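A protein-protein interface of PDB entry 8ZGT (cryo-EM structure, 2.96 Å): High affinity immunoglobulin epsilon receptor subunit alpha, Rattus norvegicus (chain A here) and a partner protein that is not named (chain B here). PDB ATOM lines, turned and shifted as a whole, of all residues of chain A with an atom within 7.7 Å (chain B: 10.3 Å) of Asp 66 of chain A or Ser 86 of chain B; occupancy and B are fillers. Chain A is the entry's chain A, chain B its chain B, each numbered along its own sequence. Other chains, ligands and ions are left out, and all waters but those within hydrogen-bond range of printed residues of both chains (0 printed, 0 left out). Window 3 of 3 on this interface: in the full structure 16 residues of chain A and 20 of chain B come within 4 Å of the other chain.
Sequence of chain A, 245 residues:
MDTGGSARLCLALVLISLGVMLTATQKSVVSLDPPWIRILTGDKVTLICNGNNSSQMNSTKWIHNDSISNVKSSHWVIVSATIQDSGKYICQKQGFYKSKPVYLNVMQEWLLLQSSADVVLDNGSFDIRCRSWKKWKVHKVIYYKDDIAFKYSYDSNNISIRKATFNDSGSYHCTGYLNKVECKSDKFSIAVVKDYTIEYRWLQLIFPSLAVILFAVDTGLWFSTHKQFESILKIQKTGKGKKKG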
ATOM      1  N   LYS A  61       0.422  29.770  -3.896  1.00  0.00           N
ATOM      2  CA  LYS A  61       1.499  28.841  -3.584  1.00  0.00           C
ATOM      3  C   LYS A  61       1.523  28.572  -2.083  1.00  0.00           C
ATOM      4  O   LYS A  61       1.530  29.509  -1.280  1.00  0.00           O
ATOM      5  CB  LYS A  61       2.835  29.413  -4.062  1.00  0.00           C
ATOM      6  CG  LYS A  61       4.077  28.759  -3.495  1.00  0.00           C
ATOM      7  CD  LYS A  61       5.309  29.263  -4.235  1.00  0.00           C
ATOM      8  CE  LYS A  61       6.482  29.494  -3.297  1.00  0.00           C
ATOM      9  NZ  LYS A  61       7.649  30.093  -4.001  1.00  0.00           N
ATOM     10  N   ILE A  63       3.275  26.402   1.219  1.00  0.00           N
ATOM     11  CA  ILE A  63       4.473  25.747   1.735  1.00  0.00           C
ATOM     12  C   ILE A  63       4.134  25.118   3.079  1.00  0.00           C
ATOM     13  O   ILE A  63       3.649  25.805   3.984  1.00  0.00           O
ATOM     14  CB  ILE A  63       5.645  26.738   1.877  1.00  0.00           C
ATOM     15  CG1 ILE A  63       6.066  27.279   0.512  1.00  0.00           C
ATOM     16  CG2 ILE A  63       6.828  26.084   2.564  1.00  0.00           C
ATOM     17  CD1 ILE A  63       5.713  28.729   0.300  1.00  0.00           C
ATOM     18  N   HIS A  64       4.387  23.817   3.209  1.00  0.00           N
ATOM     19  CA  HIS A  64       4.153  23.093   4.452  1.00  0.00           C
ATOM     20  C   HIS A  64       5.412  22.333   4.837  1.00  0.00           C
ATOM     21  O   HIS A  64       5.921  21.541   4.037  1.00  0.00           O
ATOM     22  CB  HIS A  64       2.970  22.127   4.320  1.00  0.00           C
ATOM     23  CG  HIS A  64       2.765  21.251   5.516  1.00  0.00           C
ATOM     24  ND1 HIS A  64       2.895  21.710   6.809  1.00  0.00           N
ATOM     25  CD2 HIS A  64       2.431  19.943   5.616  1.00  0.00           C
ATOM     26  CE1 HIS A  64       2.655  20.722   7.652  1.00  0.00           C
ATOM     27  NE2 HIS A  64       2.371  19.639   6.954  1.00  0.00           N
ATOM     28  N   ASN A  65       5.888  22.571   6.069  1.00  0.00           N
ATOM     29  CA  ASN A  65       7.086  21.945   6.649  1.00  0.00           C
ATOM     30  C   ASN A  65       8.320  22.159   5.771  1.00  0.00           C
ATOM     31  O   ASN A  65       9.099  21.233   5.532  1.00  0.00           O
ATOM     32  CB  ASN A  65       6.865  20.453   6.916  1.00  0.00           C
ATOM     33  CG  ASN A  65       6.369  20.171   8.322  1.00  0.00           C
ATOM     34  OD1 ASN A  65       6.326  21.056   9.173  1.00  0.00           O
ATOM     35  ND2 ASN A  65       5.994  18.920   8.566  1.00  0.00           N
ATOM     36  N   ASP A  66       8.479  23.403   5.294  1.00  0.00           N
ATOM     37  CA  ASP A  66       9.560  23.830   4.390  1.00  0.00           C
ATOM     38  C   ASP A  66       9.595  22.999   3.107  1.00  0.00           C
ATOM     39  O   ASP A  66      10.663  22.627   2.617  1.00  0.00           O
ATOM     40  CB  ASP A  66      10.927  23.811   5.085  1.00  0.00           C
ATOM     41  CG  ASP A  66      10.895  24.451   6.456  1.00  0.00           C
ATOM     42  OD1 ASP A  66      10.650  25.673   6.539  1.00  0.00           O
ATOM     43  OD2 ASP A  66      11.120  23.734   7.453  1.00  0.00           O
ATOM     44  N   SER A  67       8.420  22.704   2.558  1.00  0.00           N
ATOM     45  CA  SER A  67       8.321  21.923   1.334  1.00  0.00           C
ATOM     46  C   SER A  67       7.085  22.358   0.561  1.00  0.00           C
ATOM     47  O   SER A  67       6.037  22.623   1.154  1.00  0.00           O
ATOM     48  CB  SER A  67       8.258  20.421   1.630  1.00  0.00           C
ATOM     49  OG  SER A  67       9.477  19.959   2.184  1.00  0.00           O
ATOM     50  N   ILE A  68       7.216  22.416  -0.759  1.00  0.00           N
ATOM     51  CA  ILE A  68       6.130  22.874  -1.619  1.00  0.00           C
ATOM     52  C   ILE A  68       5.080  21.775  -1.718  1.00  0.00           C
ATOM     53  O   ILE A  68       5.395  20.624  -2.044  1.00  0.00           O
ATOM     54  CB  ILE A  68       6.669  23.267  -3.005  1.00  0.00           C
ATOM     55  CG1 ILE A  68       7.373  24.624  -2.932  1.00  0.00           C
ATOM     56  CG2 ILE A  68       5.562  23.269  -4.064  1.00  0.00           C
ATOM     57  CD1 ILE A  68       6.438  25.808  -2.926  1.00  0.00           C
ATOM     58  N   SER A  69       3.832  22.124  -1.422  1.00  0.00           N
ATOM     59  CA  SER A  69       2.724  21.191  -1.545  1.00  0.00           C
ATOM     60  C   SER A  69       2.106  21.277  -2.940  1.00  0.00           C
ATOM     61  O   SER A  69       2.371  22.199  -3.713  1.00  0.00           O
ATOM     62  CB  SER A  69       1.669  21.470  -0.477  1.00  0.00           C
ATOM     63  OG  SER A  69       0.600  22.229  -1.008  1.00  0.00           O
ATOM     64  N   GLY A  87       2.342  21.060  11.239  1.00  0.00           N
ATOM     65  CA  GLY A  87       3.559  21.792  10.952  1.00  0.00           C
ATOM     66  C   GLY A  87       3.432  23.296  10.822  1.00  0.00           C
ATOM     67  O   GLY A  87       2.760  23.952  11.620  1.00  0.00           O
ATOM     68  N   LYS A  88       4.089  23.842   9.802  1.00  0.00           N
ATOM     69  CA  LYS A  88       4.206  25.273   9.566  1.00  0.00           C
ATOM     70  C   LYS A  88       3.657  25.592   8.183  1.00  0.00           C
ATOM     71  O   LYS A  88       3.904  24.851   7.229  1.00  0.00           O
ATOM     72  CB  LYS A  88       5.670  25.702   9.668  1.00  0.00           C
ATOM     73  CG  LYS A  88       5.908  27.127  10.100  1.00  0.00           C
ATOM     74  CD  LYS A  88       7.131  27.679   9.395  1.00  0.00           C
ATOM     75  CE  LYS A  88       8.404  27.025   9.893  1.00  0.00           C
ATOM     76  NZ  LYS A  88       9.520  28.002   9.997  1.00  0.00           N
ATOM     77  N   TYR A  89       2.913  26.690   8.067  1.00  0.00           N
ATOM     78  CA  TYR A  89       2.200  27.006   6.835  1.00  0.00           C
ATOM     79  C   TYR A  89       2.501  28.430   6.392  1.00  0.00           C
ATOM     80  O   TYR A  89       2.426  29.363   7.195  1.00  0.00           O
ATOM     81  CB  TYR A  89       0.690  26.822   7.015  1.00  0.00           C
ATOM     82  CG  TYR A  89       0.271  25.382   7.182  1.00  0.00           C
ATOM     83  CD1 TYR A  89       0.201  24.799   8.441  1.00  0.00           C
ATOM     84  CD2 TYR A  89      -0.052  24.602   6.081  1.00  0.00           C
ATOM     85  CE1 TYR A  89      -0.179  23.483   8.599  1.00  0.00           C
ATOM     86  CE2 TYR A  89      -0.434  23.285   6.228  1.00  0.00           C
ATOM     87  CZ  TYR A  89      -0.495  22.731   7.488  1.00  0.00           C
ATOM     88  OH  TYR A  89      -0.876  21.420   7.636  1.00  0.00           O
ATOM     89  N   ILE A  90       2.840  28.590   5.112  1.00  0.00           N
ATOM     90  CA  ILE A  90       3.103  29.888   4.496  1.00  0.00           C
ATOM     91  C   ILE A  90       2.370  29.923   3.159  1.00  0.00           C
ATOM     92  O   ILE A  90       2.572  29.039   2.319  1.00  0.00           O
ATOM     93  CB  ILE A  90       4.611  30.133   4.291  1.00  0.00           C
ATOM     94  CG1 ILE A  90       5.325  30.324   5.629  1.00  0.00           C
ATOM     95  CG2 ILE A  90       4.854  31.343   3.411  1.00  0.00           C
ATOM     96  CD1 ILE A  90       6.820  30.365   5.514  1.00  0.00           C
ATOM     97  N   LYS A  98       5.595  36.538   0.519  1.00  0.00           N
ATOM     98  CA  LYS A  98       5.267  35.420   1.387  1.00  0.00           C
ATOM     99  C   LYS A  98       4.674  35.923   2.699  1.00  0.00           C
ATOM    100  O   LYS A  98       4.833  37.084   3.083  1.00  0.00           O
ATOM    101  CB  LYS A  98       6.503  34.564   1.656  1.00  0.00           C
ATOM    102  CG  LYS A  98       6.893  33.679   0.492  1.00  0.00           C
ATOM    103  CD  LYS A  98       7.931  32.655   0.889  1.00  0.00           C
ATOM    104  CE  LYS A  98       8.460  31.928  -0.329  1.00  0.00           C
ATOM    105  NZ  LYS A  98       9.611  31.051  -0.002  1.00  0.00           N
ATOM    106  N   SER A  99       3.980  35.029   3.387  1.00  0.00           N
ATOM    107  CA  SER A  99       3.233  35.377   4.583  1.00  0.00           C
ATOM    108  C   SER A  99       4.049  35.111   5.842  1.00  0.00           C
ATOM    109  O   SER A  99       5.058  34.403   5.829  1.00  0.00           O
ATOM    110  CB  SER A  99       1.923  34.591   4.636  1.00  0.00           C
ATOM    111  OG  SER A  99       2.148  33.282   5.119  1.00  0.00           O
ATOM    112  N   VAL B  79      24.870  33.187   5.839  1.00  0.00           N
ATOM    113  CA  VAL B  79      23.574  33.182   5.167  1.00  0.00           C
ATOM    114  C   VAL B  79      23.216  31.771   4.708  1.00  0.00           C
ATOM    115  O   VAL B  79      22.049  31.362   4.764  1.00  0.00           O
ATOM    116  CB  VAL B  79      23.583  34.192   4.001  1.00  0.00           C
ATOM    117  CG1 VAL B  79      22.241  34.233   3.283  1.00  0.00           C
ATOM    118  CG2 VAL B  79      23.924  35.575   4.518  1.00  0.00           C
ATOM    119  N   CYS B  80      24.217  30.999   4.270  1.00  0.00           N
ATOM    120  CA  CYS B  80      23.978  29.615   3.868  1.00  0.00           C
ATOM    121  C   CYS B  80      23.579  28.740   5.052  1.00  0.00           C
ATOM    122  O   CYS B  80      22.714  27.867   4.922  1.00  0.00           O
ATOM    123  CB  CYS B  80      25.224  29.051   3.186  1.00  0.00           C
ATOM    124  SG  CYS B  80      25.178  27.272   2.856  1.00  0.00           S
ATOM    125  N   SER B  81      24.188  28.966   6.215  1.00  0.00           N
ATOM    126  CA  SER B  81      23.977  28.075   7.351  1.00  0.00           C
ATOM    127  C   SER B  81      22.790  28.480   8.223  1.00  0.00           C
ATOM    128  O   SER B  81      21.900  27.661   8.476  1.00  0.00           O
ATOM    129  CB  SER B  81      25.251  28.008   8.200  1.00  0.00           C
ATOM    130  OG  SER B  81      25.116  28.769   9.387  1.00  0.00           O
ATOM    131  N   THR B  82      22.758  29.732   8.690  1.00  0.00           N
ATOM    132  CA  THR B  82      21.801  30.127   9.720  1.00  0.00           C
ATOM    133  C   THR B  82      20.388  30.317   9.175  1.00  0.00           C
ATOM    134  O   THR B  82      19.412  29.974   9.851  1.00  0.00           O
ATOM    135  CB  THR B  82      22.269  31.413  10.400  1.00  0.00           C
ATOM    136  OG1 THR B  82      22.507  32.420   9.409  1.00  0.00           O
ATOM    137  CG2 THR B  82      23.548  31.168  11.180  1.00  0.00           C
ATOM    138  N   LEU B  83      20.253  30.861   7.968  1.00  0.00           N
ATOM    139  CA  LEU B  83      18.948  31.284   7.475  1.00  0.00           C
ATOM    140  C   LEU B  83      18.174  30.116   6.878  1.00  0.00           C
ATOM    141  O   LEU B  83      18.715  29.337   6.087  1.00  0.00           O
ATOM    142  CB  LEU B  83      19.107  32.390   6.432  1.00  0.00           C
ATOM    143  CG  LEU B  83      19.147  33.830   6.948  1.00  0.00           C
ATOM    144  CD1 LEU B  83      19.133  34.811   5.790  1.00  0.00           C
ATOM    145  CD2 LEU B  83      17.991  34.101   7.890  1.00  0.00           C
ATOM    146  N   GLN B  84      16.903  30.001   7.262  1.00  0.00           N
ATOM    147  CA  GLN B  84      15.959  29.091   6.613  1.00  0.00           C
ATOM    148  C   GLN B  84      15.343  29.847   5.444  1.00  0.00           C
ATOM    149  O   GLN B  84      14.395  30.616   5.617  1.00  0.00           O
ATOM    150  CB  GLN B  84      14.899  28.615   7.599  1.00  0.00           C
ATOM    151  CG  GLN B  84      13.923  27.597   7.029  1.00  0.00           C
ATOM    152  CD  GLN B  84      14.598  26.307   6.612  1.00  0.00           C
ATOM    153  OE1 GLN B  84      14.723  26.014   5.423  1.00  0.00           O
ATOM    154  NE2 GLN B  84      15.034  25.524   7.592  1.00  0.00           N
ATOM    155  N   THR B  85      15.877  29.623   4.244  1.00  0.00           N
ATOM    156  CA  THR B  85      15.561  30.458   3.092  1.00  0.00           C
ATOM    157  C   THR B  85      14.180  30.199   2.504  1.00  0.00           C
ATOM    158  O   THR B  85      13.748  30.967   1.638  1.00  0.00           O
ATOM    159  CB  THR B  85      16.616  30.267   1.999  1.00  0.00           C
ATOM    160  OG1 THR B  85      16.543  28.931   1.489  1.00  0.00           O
ATOM    161  CG2 THR B  85      18.008  30.517   2.555  1.00  0.00           C
ATOM    162  N   SER B  86      13.479  29.152   2.937  1.00  0.00           N
ATOM    163  CA  SER B  86      12.149  28.879   2.407  1.00  0.00           C
ATOM    164  C   SER B  86      11.072  29.768   3.013  1.00  0.00           C
ATOM    165  O   SER B  86       9.947  29.776   2.508  1.00  0.00           O
ATOM    166  CB  SER B  86      11.782  27.410   2.624  1.00  0.00           C
ATOM    167  OG  SER B  86      12.157  26.972   3.918  1.00  0.00           O
ATOM    168  N   ASP B  87      11.385  30.507   4.077  1.00  0.00           N
ATOM    169  CA  ASP B  87      10.434  31.415   4.701  1.00  0.00           C
ATOM    170  C   ASP B  87      10.475  32.819   4.117  1.00  0.00           C
ATOM    171  O   ASP B  87       9.564  33.610   4.387  1.00  0.00           O
ATOM    172  CB  ASP B  87      10.697  31.497   6.208  1.00  0.00           C
ATOM    173  CG  ASP B  87      10.493  30.172   6.909  1.00  0.00           C
ATOM    174  OD1 ASP B  87      10.201  29.171   6.223  1.00  0.00           O
ATOM    175  OD2 ASP B  87      10.624  30.131   8.150  1.00  0.00           O
ATOM    176  N   PHE B  88      11.495  33.147   3.328  1.00  0.00           N
ATOM    177  CA  PHE B  88      11.692  34.488   2.807  1.00  0.00           C
ATOM    178  C   PHE B  88      11.631  34.475   1.286  1.00  0.00           C
ATOM    179  O   PHE B  88      11.824  33.440   0.643  1.00  0.00           O
ATOM    180  CB  PHE B  88      13.029  35.071   3.283  1.00  0.00           C
ATOM    181  CG  PHE B  88      13.291  34.854   4.744  1.00  0.00           C
ATOM    182  CD1 PHE B  88      12.559  35.541   5.701  1.00  0.00           C
ATOM    183  CD2 PHE B  88      14.259  33.956   5.162  1.00  0.00           C
ATOM    184  CE1 PHE B  88      12.791  35.340   7.048  1.00  0.00           C
ATOM    185  CE2 PHE B  88      14.497  33.751   6.508  1.00  0.00           C
ATOM    186  CZ  PHE B  88      13.762  34.443   7.451  1.00  0.00           C
ATOM    187  N   ASP B  89      11.357  35.648   0.722  1.00  0.00           N
ATOM    188  CA  ASP B  89      11.131  35.781  -0.708  1.00  0.00           C
ATOM    189  C   ASP B  89      12.434  35.645  -1.488  1.00  0.00           C
ATOM    190  O   ASP B  89      13.531  35.864  -0.969  1.00  0.00           O
ATOM    191  CB  ASP B  89      10.484  37.127  -1.020  1.00  0.00           C
ATOM    192  CG  ASP B  89       9.036  37.183  -0.604  1.00  0.00           C
ATOM    193  OD1 ASP B  89       8.770  37.391   0.597  1.00  0.00           O
ATOM    194  OD2 ASP B  89       8.162  37.018  -1.480  1.00  0.00           O
ATOM    195  N   ASP B  90      12.298  35.273  -2.760  1.00  0.00           N
ATOM    196  CA  ASP B  90      13.445  35.182  -3.652  1.00  0.00           C
ATOM    197  C   ASP B  90      13.835  36.527  -4.249  1.00  0.00           C
ATOM    198  O   ASP B  90      14.914  36.633  -4.839  1.00  0.00           O
ATOM    199  CB  ASP B  90      13.161  34.183  -4.774  1.00  0.00           C
ATOM    200  CG  ASP B  90      12.576  32.885  -4.260  1.00  0.00           C
ATOM    201  OD1 ASP B  90      12.994  32.434  -3.173  1.00  0.00           O
ATOM    202  OD2 ASP B  90      11.697  32.316  -4.941  1.00  0.00           O
ATOM    203  N   LEU B  93      16.410  37.807  -1.523  1.00  0.00           N
ATOM    204  CA  LEU B  93      17.623  37.001  -1.486  1.00  0.00           C
ATOM    205  C   LEU B  93      18.232  36.793  -2.864  1.00  0.00           C
ATOM    206  O   LEU B  93      18.784  35.720  -3.134  1.00  0.00           O
ATOM    207  CB  LEU B  93      17.330  35.652  -0.827  1.00  0.00           C
ATOM    208  CG  LEU B  93      17.062  35.660   0.677  1.00  0.00           C
ATOM    209  CD1 LEU B  93      16.275  34.428   1.078  1.00  0.00           C
ATOM    210  CD2 LEU B  93      18.363  35.739   1.454  1.00  0.00           C
ATOM    211  N   TYR B  96      21.884  35.803  -3.131  1.00  0.00           N
ATOM    212  CA  TYR B  96      22.193  34.433  -2.747  1.00  0.00           C
ATOM    213  C   TYR B  96      21.771  33.419  -3.800  1.00  0.00           C
ATOM    214  O   TYR B  96      22.477  32.429  -4.020  1.00  0.00           O
ATOM    215  CB  TYR B  96      21.522  34.091  -1.416  1.00  0.00           C
ATOM    216  CG  TYR B  96      21.954  32.760  -0.854  1.00  0.00           C
ATOM    217  CD1 TYR B  96      21.021  31.884  -0.311  1.00  0.00           C
ATOM    218  CD2 TYR B  96      23.288  32.371  -0.876  1.00  0.00           C
ATOM    219  CE1 TYR B  96      21.404  30.660   0.196  1.00  0.00           C
ATOM    220  CE2 TYR B  96      23.682  31.148  -0.369  1.00  0.00           C
ATOM    221  CZ  TYR B  96      22.734  30.299   0.166  1.00  0.00           C
ATOM    222  OH  TYR B  96      23.112  29.079   0.670  1.00  0.00           O
ATOM    223  N   ARG B  97      20.627  33.640  -4.452  1.00  0.00           N
ATOM    224  CA  ARG B  97      20.162  32.719  -5.481  1.00  0.00           C
ATOM    225  C   ARG B  97      21.008  32.794  -6.743  1.00  0.00           C
ATOM    226  O   ARG B  97      21.060  31.819  -7.498  1.00  0.00           O
ATOM    227  CB  ARG B  97      18.692  32.992  -5.803  1.00  0.00           C
ATOM    228  CG  ARG B  97      17.793  32.929  -4.583  1.00  0.00           C
ATOM    229  CD  ARG B  97      16.543  32.113  -4.838  1.00  0.00           C
ATOM    230  NE  ARG B  97      15.813  31.842  -3.605  1.00  0.00           N
ATOM    231  CZ  ARG B  97      16.116  30.880  -2.744  1.00  0.00           C
ATOM    232  NH1 ARG B  97      17.131  30.058  -2.953  1.00  0.00           N
ATOM    233  NH2 ARG B  97      15.379  30.737  -1.645  1.00  0.00           N
ATOM    234  N   VAL B 173      14.948  40.689   8.480  1.00  0.00           N
ATOM    235  CA  VAL B 173      15.855  39.961   7.597  1.00  0.00           C
ATOM    236  C   VAL B 173      16.163  40.784   6.347  1.00  0.00           C
ATOM    237  O   VAL B 173      17.308  40.809   5.876  1.00  0.00           O
ATOM    238  CB  VAL B 173      15.263  38.572   7.277  1.00  0.00           C
ATOM    239  CG1 VAL B 173      15.785  37.996   5.965  1.00  0.00           C
ATOM    240  CG2 VAL B 173      15.560  37.607   8.416  1.00  0.00           C
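Hydrophobic or aromatic side chains of chain A that line the printed part of chain B: Ile 90. Printed residues of chain B that touch a printed residue of chain A: Gln 84, Ser 86, Asp 87, Phe 88 and Asp 89. Among the printed residues, Asp or Glu carboxylates within 4 Å of a Lys or Arg side-chain nitrogen of the other chain: Lys 88 of chain A with Asp 87 of chain B.
OD1 of Asp 66 of chain A touches CG of Gln 84 of chain B, 3.8 Å away. OD1 of Asp 66 of chain A touches OD1 of Asp 87 of chain B (3.5 Å). Asp 87 of chain B touches Ile 90 of chain A (OD1 to CD1, 3.7 Å). Lys 98 of chain A touches Asp 87 of chain B (CD to O, 3.98 Å).
The backbone NH of Ile 63 of chain A sits at hydrogen-bond distance from the backbone carbonyl oxygen of Ile 90 of chain A, 2.9 Å away. A ring nitrogen (ND1) of His 64 of chain A sits close to the backbone carbonyl oxygen (O) of Lys 88 of chain A (3.3 Å). N of Asn 65 of chain A sits at hydrogen-bond distance from O of Lys 88 of chain A (3.2 Å). The side-chain hydroxyl of Ser 86 of chain B lies within hydrogen-bond range of the side-chain amide oxygen of Gln 84 of chain B, 3.1 Å away.
Of chain B, only Gln 84 (3.8 Å), Ser 86 (3.3 Å) and Asp 87 (3.5 Å) come within 4 Å of Asp 66 of chain A. Of chain A, only Asp 66 and Lys 98 come within 4 Å of Ser 86 of chain B. No residue of chain B comes within 4 Å of Asn 65 of chain A. Of the printed residues of chain A, Asp 89 of chain B touches Lys 98. Printed residues of chain A within 4 Å of Phe 88 of chain B: Lys 98. Printed residues of chain A within 4 Å of Asp 87 of chain B: Asp 66 (3.5 Å), Lys 88 (3.0 Å), Ile 90 (3.7 Å) and Lys 98 (3.98 Å). Printed residues of chain B within 4 Å of Lys 98 of chain A: Ser 86, Asp 87, Phe 88 and Asp 89. Printed residues of chain B within 4 Å of Ile 90 of chain A: Asp 87 (3.7 Å). Lys 61 of chain A touches none of the printed residues of chain B. Cys 80 of chain B touches none of the printed residues of chain A. The nearest residue of chain B that does not touch Asp 66 of chain A is Thr 85 of chain B (6.9 Å). The nearest residue of chain A that does not touch Ser 86 of chain B is Ile 90 of chain A (4.4 Å).
OD1 of Asp 66 of chain A sits at hydrogen-bond distance from OG of Ser 86 of chain B (3.3 Å). NZ of Lys 88 of chain A is in salt-bridge range of OD2 of Asp 87 of chain B, at 3.0 Å. O of Ser 86 of chain B sits at hydrogen-bond distance from NZ of Lys 98 of chain A (2.8 Å). O of Phe 88 of chain B lies within hydrogen-bond range of NZ of Lys 98 of chain A (3.3 Å). The side-chain carboxylate (OD1) of Asp 89 of chain B is in hydrogen-bond range of the backbone NH (N) of Lys 98 of chain A (3.3 Å).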
